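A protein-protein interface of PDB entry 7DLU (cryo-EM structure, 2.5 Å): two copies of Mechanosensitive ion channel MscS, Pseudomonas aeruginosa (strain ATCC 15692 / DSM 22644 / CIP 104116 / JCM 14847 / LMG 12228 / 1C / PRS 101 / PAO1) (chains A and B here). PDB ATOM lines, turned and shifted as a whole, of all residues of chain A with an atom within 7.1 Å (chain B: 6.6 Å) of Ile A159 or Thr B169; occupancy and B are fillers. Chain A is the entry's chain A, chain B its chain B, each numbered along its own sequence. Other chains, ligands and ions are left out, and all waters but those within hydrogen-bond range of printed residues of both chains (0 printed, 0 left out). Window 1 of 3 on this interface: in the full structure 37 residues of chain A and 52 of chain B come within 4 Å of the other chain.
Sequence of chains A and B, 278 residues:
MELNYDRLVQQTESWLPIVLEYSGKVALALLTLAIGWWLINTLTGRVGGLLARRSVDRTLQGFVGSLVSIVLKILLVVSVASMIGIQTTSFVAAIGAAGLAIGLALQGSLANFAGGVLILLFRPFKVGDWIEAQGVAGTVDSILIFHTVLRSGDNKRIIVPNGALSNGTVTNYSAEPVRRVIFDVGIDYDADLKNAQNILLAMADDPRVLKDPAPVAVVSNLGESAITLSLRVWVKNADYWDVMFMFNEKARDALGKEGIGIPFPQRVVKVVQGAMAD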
ATOM      1  N   ALA A 133      27.904  19.517 -18.180  1.00  0.00           N
ATOM      2  CA  ALA A 133      29.217  20.112 -18.009  1.00  0.00           C
ATOM      3  C   ALA A 133      29.688  19.860 -16.589  1.00  0.00           C
ATOM      4  O   ALA A 133      28.880  19.767 -15.666  1.00  0.00           O
ATOM      5  CB  ALA A 133      29.191  21.613 -18.301  1.00  0.00           C
ATOM      6  N   GLN A 134      31.006  19.751 -16.428  1.00  0.00           N
ATOM      7  CA  GLN A 134      31.655  19.621 -15.125  1.00  0.00           C
ATOM      8  C   GLN A 134      31.213  18.373 -14.370  1.00  0.00           C
ATOM      9  O   GLN A 134      31.240  18.350 -13.137  1.00  0.00           O
ATOM     10  CB  GLN A 134      31.422  20.865 -14.259  1.00  0.00           C
ATOM     11  CG  GLN A 134      31.899  22.164 -14.884  1.00  0.00           C
ATOM     12  CD  GLN A 134      33.393  22.192 -15.106  1.00  0.00           C
ATOM     13  OE1 GLN A 134      34.166  21.766 -14.253  1.00  0.00           O
ATOM     14  NE2 GLN A 134      33.809  22.693 -16.260  1.00  0.00           N
ATOM     15  N   GLY A 135      30.802  17.331 -15.083  1.00  0.00           N
ATOM     16  CA  GLY A 135      30.387  16.097 -14.454  1.00  0.00           C
ATOM     17  C   GLY A 135      28.935  16.025 -14.040  1.00  0.00           C
ATOM     18  O   GLY A 135      28.529  15.017 -13.455  1.00  0.00           O
ATOM     19  N   VAL A 136      28.139  17.057 -14.321  1.00  0.00           N
ATOM     20  CA  VAL A 136      26.721  17.070 -13.994  1.00  0.00           C
ATOM     21  C   VAL A 136      25.936  17.375 -15.261  1.00  0.00           C
ATOM     22  O   VAL A 136      26.500  17.705 -16.305  1.00  0.00           O
ATOM     23  CB  VAL A 136      26.377  18.086 -12.881  1.00  0.00           C
ATOM     24  CG1 VAL A 136      26.971  17.647 -11.564  1.00  0.00           C
ATOM     25  CG2 VAL A 136      26.873  19.466 -13.245  1.00  0.00           C
ATOM     26  N   PHE A 146      27.475  34.794 -10.763  1.00  0.00           N
ATOM     27  CA  PHE A 146      28.392  33.994  -9.962  1.00  0.00           C
ATOM     28  C   PHE A 146      28.254  32.496 -10.222  1.00  0.00           C
ATOM     29  O   PHE A 146      29.260  31.785 -10.283  1.00  0.00           O
ATOM     30  CB  PHE A 146      28.194  34.283  -8.476  1.00  0.00           C
ATOM     31  CG  PHE A 146      29.162  33.557  -7.599  1.00  0.00           C
ATOM     32  CD1 PHE A 146      30.478  33.971  -7.515  1.00  0.00           C
ATOM     33  CD2 PHE A 146      28.765  32.445  -6.876  1.00  0.00           C
ATOM     34  CE1 PHE A 146      31.375  33.299  -6.720  1.00  0.00           C
ATOM     35  CE2 PHE A 146      29.658  31.766  -6.082  1.00  0.00           C
ATOM     36  CZ  PHE A 146      30.965  32.195  -6.002  1.00  0.00           C
ATOM     37  N   HIS A 147      27.027  31.995 -10.364  1.00  0.00           N
ATOM     38  CA  HIS A 147      26.816  30.574 -10.601  1.00  0.00           C
ATOM     39  C   HIS A 147      25.616  30.368 -11.514  1.00  0.00           C
ATOM     40  O   HIS A 147      24.846  31.287 -11.794  1.00  0.00           O
ATOM     41  CB  HIS A 147      26.627  29.801  -9.290  1.00  0.00           C
ATOM     42  CG  HIS A 147      25.519  30.323  -8.429  1.00  0.00           C
ATOM     43  ND1 HIS A 147      24.194  30.263  -8.800  1.00  0.00           N
ATOM     44  CD2 HIS A 147      25.541  30.906  -7.209  1.00  0.00           C
ATOM     45  CE1 HIS A 147      23.447  30.790  -7.848  1.00  0.00           C
ATOM     46  NE2 HIS A 147      24.240  31.187  -6.870  1.00  0.00           N
ATOM     47  N   THR A 148      25.477  29.132 -11.981  1.00  0.00           N
ATOM     48  CA  THR A 148      24.359  28.687 -12.796  1.00  0.00           C
ATOM     49  C   THR A 148      23.609  27.600 -12.040  1.00  0.00           C
ATOM     50  O   THR A 148      24.219  26.785 -11.343  1.00  0.00           O
ATOM     51  CB  THR A 148      24.842  28.158 -14.154  1.00  0.00           C
ATOM     52  OG1 THR A 148      25.693  29.131 -14.769  1.00  0.00           O
ATOM     53  CG2 THR A 148      23.675  27.879 -15.080  1.00  0.00           C
ATOM     54  N   VAL A 149      22.287  27.596 -12.165  1.00  0.00           N
ATOM     55  CA  VAL A 149      21.429  26.660 -11.453  1.00  0.00           C
ATOM     56  C   VAL A 149      20.798  25.706 -12.457  1.00  0.00           C
ATOM     57  O   VAL A 149      20.289  26.129 -13.499  1.00  0.00           O
ATOM     58  CB  VAL A 149      20.352  27.398 -10.631  1.00  0.00           C
ATOM     59  CG1 VAL A 149      19.418  26.412  -9.973  1.00  0.00           C
ATOM     60  CG2 VAL A 149      21.005  28.277  -9.586  1.00  0.00           C
ATOM     61  N   LEU A 150      20.838  24.416 -12.140  1.00  0.00           N
ATOM     62  CA  LEU A 150      20.307  23.358 -12.983  1.00  0.00           C
ATOM     63  C   LEU A 150      19.301  22.543 -12.187  1.00  0.00           C
ATOM     64  O   LEU A 150      19.429  22.391 -10.973  1.00  0.00           O
ATOM     65  CB  LEU A 150      21.416  22.420 -13.482  1.00  0.00           C
ATOM     66  CG  LEU A 150      22.191  22.678 -14.772  1.00  0.00           C
ATOM     67  CD1 LEU A 150      22.568  24.128 -14.916  1.00  0.00           C
ATOM     68  CD2 LEU A 150      23.428  21.810 -14.794  1.00  0.00           C
ATOM     69  N   ARG A 157      18.401  20.162  -7.298  1.00  0.00           N
ATOM     70  CA  ARG A 157      19.005  21.418  -7.721  1.00  0.00           C
ATOM     71  C   ARG A 157      20.524  21.332  -7.667  1.00  0.00           C
ATOM     72  O   ARG A 157      21.096  20.955  -6.642  1.00  0.00           O
ATOM     73  CB  ARG A 157      18.501  22.560  -6.842  1.00  0.00           C
ATOM     74  CG  ARG A 157      19.345  23.809  -6.886  1.00  0.00           C
ATOM     75  CD  ARG A 157      18.674  24.941  -6.142  1.00  0.00           C
ATOM     76  NE  ARG A 157      17.303  25.134  -6.593  1.00  0.00           N
ATOM     77  CZ  ARG A 157      16.416  25.911  -5.983  1.00  0.00           C
ATOM     78  NH1 ARG A 157      15.189  26.022  -6.465  1.00  0.00           N
ATOM     79  NH2 ARG A 157      16.755  26.571  -4.888  1.00  0.00           N
ATOM     80  N   ILE A 158      21.171  21.695  -8.771  1.00  0.00           N
ATOM     81  CA  ILE A 158      22.623  21.676  -8.898  1.00  0.00           C
ATOM     82  C   ILE A 158      23.102  23.103  -9.109  1.00  0.00           C
ATOM     83  O   ILE A 158      22.525  23.842  -9.910  1.00  0.00           O
ATOM     84  CB  ILE A 158      23.075  20.766 -10.054  1.00  0.00           C
ATOM     85  CG1 ILE A 158      22.463  19.374  -9.901  1.00  0.00           C
ATOM     86  CG2 ILE A 158      24.585  20.680 -10.110  1.00  0.00           C
ATOM     87  CD1 ILE A 158      22.456  18.571 -11.163  1.00  0.00           C
ATOM     88  N   ILE A 159      24.142  23.495  -8.382  1.00  0.00           N
ATOM     89  CA  ILE A 159      24.725  24.827  -8.488  1.00  0.00           C
ATOM     90  C   ILE A 159      26.141  24.669  -9.013  1.00  0.00           C
ATOM     91  O   ILE A 159      26.970  24.009  -8.376  1.00  0.00           O
ATOM     92  CB  ILE A 159      24.716  25.567  -7.142  1.00  0.00           C
ATOM     93  CG1 ILE A 159      23.283  25.815  -6.676  1.00  0.00           C
ATOM     94  CG2 ILE A 159      25.454  26.881  -7.255  1.00  0.00           C
ATOM     95  CD1 ILE A 159      22.822  24.861  -5.605  1.00  0.00           C
ATOM     96  N   VAL A 160      26.418  25.263 -10.167  1.00  0.00           N
ATOM     97  CA  VAL A 160      27.710  25.152 -10.835  1.00  0.00           C
ATOM     98  C   VAL A 160      28.346  26.534 -10.864  1.00  0.00           C
ATOM     99  O   VAL A 160      27.740  27.469 -11.387  1.00  0.00           O
ATOM    100  CB  VAL A 160      27.588  24.593 -12.264  1.00  0.00           C
ATOM    101  CG1 VAL A 160      28.957  24.279 -12.824  1.00  0.00           C
ATOM    102  CG2 VAL A 160      26.709  23.363 -12.277  1.00  0.00           C
ATOM    103  N   PRO A 161      29.552  26.709 -10.334  1.00  0.00           N
ATOM    104  CA  PRO A 161      30.229  28.004 -10.455  1.00  0.00           C
ATOM    105  C   PRO A 161      30.581  28.314 -11.902  1.00  0.00           C
ATOM    106  O   PRO A 161      30.869  27.422 -12.701  1.00  0.00           O
ATOM    107  CB  PRO A 161      31.485  27.827  -9.599  1.00  0.00           C
ATOM    108  CG  PRO A 161      31.720  26.360  -9.577  1.00  0.00           C
ATOM    109  CD  PRO A 161      30.368  25.723  -9.608  1.00  0.00           C
ATOM    110  N   ARG B 123      22.888  32.062  -1.097  1.00  0.00           N
ATOM    111  CA  ARG B 123      22.610  30.912  -0.248  1.00  0.00           C
ATOM    112  C   ARG B 123      22.296  29.672  -1.075  1.00  0.00           C
ATOM    113  O   ARG B 123      21.143  29.472  -1.473  1.00  0.00           O
ATOM    114  CB  ARG B 123      21.450  31.223   0.695  1.00  0.00           C
ATOM    115  CG  ARG B 123      21.517  32.608   1.302  1.00  0.00           C
ATOM    116  CD  ARG B 123      20.237  32.947   2.035  1.00  0.00           C
ATOM    117  NE  ARG B 123      20.094  34.383   2.247  1.00  0.00           N
ATOM    118  CZ  ARG B 123      20.347  34.996   3.398  1.00  0.00           C
ATOM    119  NH1 ARG B 123      20.752  34.297   4.448  1.00  0.00           N
ATOM    120  NH2 ARG B 123      20.192  36.308   3.501  1.00  0.00           N
ATOM    121  N   PRO B 124      23.282  28.808  -1.344  1.00  0.00           N
ATOM    122  CA  PRO B 124      23.002  27.599  -2.126  1.00  0.00           C
ATOM    123  C   PRO B 124      22.274  26.559  -1.298  1.00  0.00           C
ATOM    124  O   PRO B 124      21.485  25.769  -1.824  1.00  0.00           O
ATOM    125  CB  PRO B 124      24.397  27.111  -2.541  1.00  0.00           C
ATOM    126  CG  PRO B 124      25.375  28.107  -1.975  1.00  0.00           C
ATOM    127  CD  PRO B 124      24.674  28.824  -0.883  1.00  0.00           C
ATOM    128  N   PHE B 125      22.539  26.551   0.005  1.00  0.00           N
ATOM    129  CA  PHE B 125      21.917  25.602   0.911  1.00  0.00           C
ATOM    130  C   PHE B 125      21.702  26.274   2.257  1.00  0.00           C
ATOM    131  O   PHE B 125      22.307  27.302   2.563  1.00  0.00           O
ATOM    132  CB  PHE B 125      22.760  24.328   1.068  1.00  0.00           C
ATOM    133  CG  PHE B 125      24.209  24.586   1.366  1.00  0.00           C
ATOM    134  CD1 PHE B 125      24.635  24.808   2.660  1.00  0.00           C
ATOM    135  CD2 PHE B 125      25.146  24.591   0.353  1.00  0.00           C
ATOM    136  CE1 PHE B 125      25.958  25.041   2.936  1.00  0.00           C
ATOM    137  CE2 PHE B 125      26.473  24.826   0.627  1.00  0.00           C
ATOM    138  CZ  PHE B 125      26.877  25.049   1.920  1.00  0.00           C
ATOM    139  N   GLU B 132      25.277  17.325  -1.316  1.00  0.00           N
ATOM    140  CA  GLU B 132      26.340  16.427  -1.747  1.00  0.00           C
ATOM    141  C   GLU B 132      27.361  17.239  -2.523  1.00  0.00           C
ATOM    142  O   GLU B 132      27.026  17.845  -3.544  1.00  0.00           O
ATOM    143  CB  GLU B 132      25.785  15.293  -2.605  1.00  0.00           C
ATOM    144  CG  GLU B 132      26.818  14.626  -3.479  1.00  0.00           C
ATOM    145  CD  GLU B 132      26.281  13.393  -4.166  1.00  0.00           C
ATOM    146  OE1 GLU B 132      25.634  12.568  -3.487  1.00  0.00           O
ATOM    147  OE2 GLU B 132      26.501  13.248  -5.387  1.00  0.00           O
ATOM    148  N   ALA B 133      28.602  17.251  -2.045  1.00  0.00           N
ATOM    149  CA  ALA B 133      29.646  18.054  -2.657  1.00  0.00           C
ATOM    150  C   ALA B 133      30.995  17.552  -2.180  1.00  0.00           C
ATOM    151  O   ALA B 133      31.119  17.047  -1.066  1.00  0.00           O
ATOM    152  CB  ALA B 133      29.480  19.536  -2.315  1.00  0.00           C
ATOM    153  N   GLN B 134      32.002  17.697  -3.039  1.00  0.00           N
ATOM    154  CA  GLN B 134      33.392  17.379  -2.721  1.00  0.00           C
ATOM    155  C   GLN B 134      33.591  15.912  -2.358  1.00  0.00           C
ATOM    156  O   GLN B 134      34.512  15.575  -1.610  1.00  0.00           O
ATOM    157  CB  GLN B 134      33.925  18.271  -1.593  1.00  0.00           C
ATOM    158  CG  GLN B 134      33.847  19.761  -1.880  1.00  0.00           C
ATOM    159  CD  GLN B 134      34.700  20.173  -3.058  1.00  0.00           C
ATOM    160  OE1 GLN B 134      35.831  19.721  -3.207  1.00  0.00           O
ATOM    161  NE2 GLN B 134      34.158  21.036  -3.905  1.00  0.00           N
ATOM    162  N   ALA B 164      36.934  25.347  -1.324  1.00  0.00           N
ATOM    163  CA  ALA B 164      36.656  24.344  -2.344  1.00  0.00           C
ATOM    164  C   ALA B 164      35.168  24.055  -2.451  1.00  0.00           C
ATOM    165  O   ALA B 164      34.683  23.685  -3.524  1.00  0.00           O
ATOM    166  CB  ALA B 164      37.427  23.063  -2.043  1.00  0.00           C
ATOM    167  N   LEU B 165      34.429  24.222  -1.355  1.00  0.00           N
ATOM    168  CA  LEU B 165      32.986  24.015  -1.395  1.00  0.00           C
ATOM    169  C   LEU B 165      32.311  25.051  -2.284  1.00  0.00           C
ATOM    170  O   LEU B 165      31.480  24.709  -3.131  1.00  0.00           O
ATOM    171  CB  LEU B 165      32.417  24.058   0.022  1.00  0.00           C
ATOM    172  CG  LEU B 165      30.948  23.702   0.230  1.00  0.00           C
ATOM    173  CD1 LEU B 165      30.677  22.273  -0.167  1.00  0.00           C
ATOM    174  CD2 LEU B 165      30.570  23.927   1.673  1.00  0.00           C
ATOM    175  N   SER B 166      32.665  26.326  -2.112  1.00  0.00           N
ATOM    176  CA  SER B 166      32.059  27.380  -2.915  1.00  0.00           C
ATOM    177  C   SER B 166      32.625  27.445  -4.324  1.00  0.00           C
ATOM    178  O   SER B 166      32.012  28.077  -5.189  1.00  0.00           O
ATOM    179  CB  SER B 166      32.237  28.734  -2.231  1.00  0.00           C
ATOM    180  OG  SER B 166      33.592  29.132  -2.256  1.00  0.00           O
ATOM    181  N   ASN B 167      33.766  26.811  -4.581  1.00  0.00           N
ATOM    182  CA  ASN B 167      34.336  26.802  -5.922  1.00  0.00           C
ATOM    183  C   ASN B 167      34.035  25.529  -6.704  1.00  0.00           C
ATOM    184  O   ASN B 167      34.619  25.327  -7.771  1.00  0.00           O
ATOM    185  CB  ASN B 167      35.847  27.016  -5.851  1.00  0.00           C
ATOM    186  CG  ASN B 167      36.223  28.479  -5.875  1.00  0.00           C
ATOM    187  OD1 ASN B 167      35.632  29.267  -6.608  1.00  0.00           O
ATOM    188  ND2 ASN B 167      37.205  28.852  -5.066  1.00  0.00           N
ATOM    189  N   GLY B 168      33.147  24.667  -6.208  1.00  0.00           N
ATOM    190  CA  GLY B 168      32.746  23.470  -6.911  1.00  0.00           C
ATOM    191  C   GLY B 168      31.235  23.376  -7.038  1.00  0.00           C
ATOM    192  O   GLY B 168      30.496  24.269  -6.620  1.00  0.00           O
ATOM    193  N   THR B 169      30.791  22.267  -7.621  1.00  0.00           N
ATOM    194  CA  THR B 169      29.363  22.037  -7.776  1.00  0.00           C
ATOM    195  C   THR B 169      28.773  21.461  -6.496  1.00  0.00           C
ATOM    196  O   THR B 169      29.413  20.686  -5.781  1.00  0.00           O
ATOM    197  CB  THR B 169      29.074  21.098  -8.949  1.00  0.00           C
ATOM    198  OG1 THR B 169      29.242  19.740  -8.535  1.00  0.00           O
ATOM    199  CG2 THR B 169      30.004  21.380 -10.108  1.00  0.00           C
ATOM    200  N   VAL B 170      27.542  21.867  -6.200  1.00  0.00           N
ATOM    201  CA  VAL B 170      26.809  21.420  -5.025  1.00  0.00           C
ATOM    202  C   VAL B 170      25.442  20.942  -5.485  1.00  0.00           C
ATOM    203  O   VAL B 170      24.730  21.673  -6.180  1.00  0.00           O
ATOM    204  CB  VAL B 170      26.659  22.538  -3.976  1.00  0.00           C
ATOM    205  CG1 VAL B 170      25.908  22.027  -2.761  1.00  0.00           C
ATOM    206  CG2 VAL B 170      28.008  23.081  -3.568  1.00  0.00           C
ATOM    207  N   THR B 171      25.083  19.720  -5.112  1.00  0.00           N
ATOM    208  CA  THR B 171      23.765  19.168  -5.397  1.00  0.00           C
ATOM    209  C   THR B 171      22.917  19.255  -4.137  1.00  0.00           C
ATOM    210  O   THR B 171      23.293  18.715  -3.096  1.00  0.00           O
ATOM    211  CB  THR B 171      23.865  17.721  -5.876  1.00  0.00           C
ATOM    212  OG1 THR B 171      24.788  17.638  -6.966  1.00  0.00           O
ATOM    213  CG2 THR B 171      22.512  17.226  -6.337  1.00  0.00           C
ATOM    214  N   ASN B 172      21.778  19.930  -4.233  1.00  0.00           N
ATOM    215  CA  ASN B 172      20.880  20.142  -3.106  1.00  0.00           C
ATOM    216  C   ASN B 172      19.634  19.291  -3.321  1.00  0.00           C
ATOM    217  O   ASN B 172      18.850  19.549  -4.238  1.00  0.00           O
ATOM    218  CB  ASN B 172      20.531  21.622  -2.970  1.00  0.00           C
ATOM    219  CG  ASN B 172      19.939  21.964  -1.625  1.00  0.00           C
ATOM    220  OD1 ASN B 172      19.476  21.093  -0.896  1.00  0.00           O
ATOM    221  ND2 ASN B 172      19.944  23.242  -1.290  1.00  0.00           N
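Leu A150 touches none of the printed residues of chain B.
Of the printed residues of chain B, Arg A157 touches Val B170, Thr B171 and Asn B172.
Of the printed residues of chain B, Ile A158 touches Val B170 (3.4 Å).
Printed residues of chain B within 4 Å of Ile A159: Gly B168 (3.9 Å), Thr B169 (3.2 Å) and Val B170 (2.9 Å).
Leu B165 touches none of the printed residues of chain A.
Of the printed residues of chain A, Gly B168 touches Ile A159 (3.9 Å) and Pro A161 (3.3 Å).
Of the printed residues of chain A, Thr B169 touches Ile A159 (3.2 Å).
Of the printed residues of chain A, Val B170 touches Arg A157 (3.7 Å), Ile A158 (3.4 Å) and Ile A159 (2.9 Å).
The nearest residue of chain B that does not touch Ile A159 is Pro B124 (4.1 Å).
The nearest printed residue of chain A that does not touch Thr B169 is Pro A161 (4.01 Å).
The backbone carbonyl oxygen (O) of Val B170 is in hydrogen-bond range of the backbone NH (N) of Ile A159.
O of Arg A157 lies within hydrogen-bond range of N of Asn B172, at 2.7 Å.
Of the 14 printed residues of chain A, 4 touch a printed residue of chain B.
Printed residues of chain A that touch a printed residue of chain B: Arg A157, Ile A158, Ile A159 and Pro A161.
Among the printed residues, 9 pairs touch across the chains.
Among the printed residues, no Asp or Glu carboxylate lies within 4 Å of a Lys or Arg side-chain nitrogen of the other chain.
Positions printed for both chains: 133 and 134.
Of the 9 pairs that touch across the chains among the printed residues, none has its exchanged pair printed and touching as well.
Val B170 touches Arg A157.
Arg A157 touches Thr B171.
CA of Ile A158 touches O of Val B170, 3.4 Å away.
Gly B168 touches Ile A159 (O to O, 3.9 Å).
Ile A159 touches Thr B169 (O to CA, 3.2 Å).
O of Asn B167 touches CG of Pro A161 (3.6 Å).
O of Gly B168 touches CD of Pro A161, at 3.3 Å.
O of Pro B124 sits at hydrogen-bond distance from ND2 of Asn B172 (3.0 Å).
The backbone NH of Glu B132 is in hydrogen-bond range of the backbone carbonyl oxygen of Thr B171 (3.0 Å).
The backbone NH (N) of Leu A150 sits at hydrogen-bond distance from the backbone carbonyl oxygen (O) of Ile A158 (2.9 Å).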
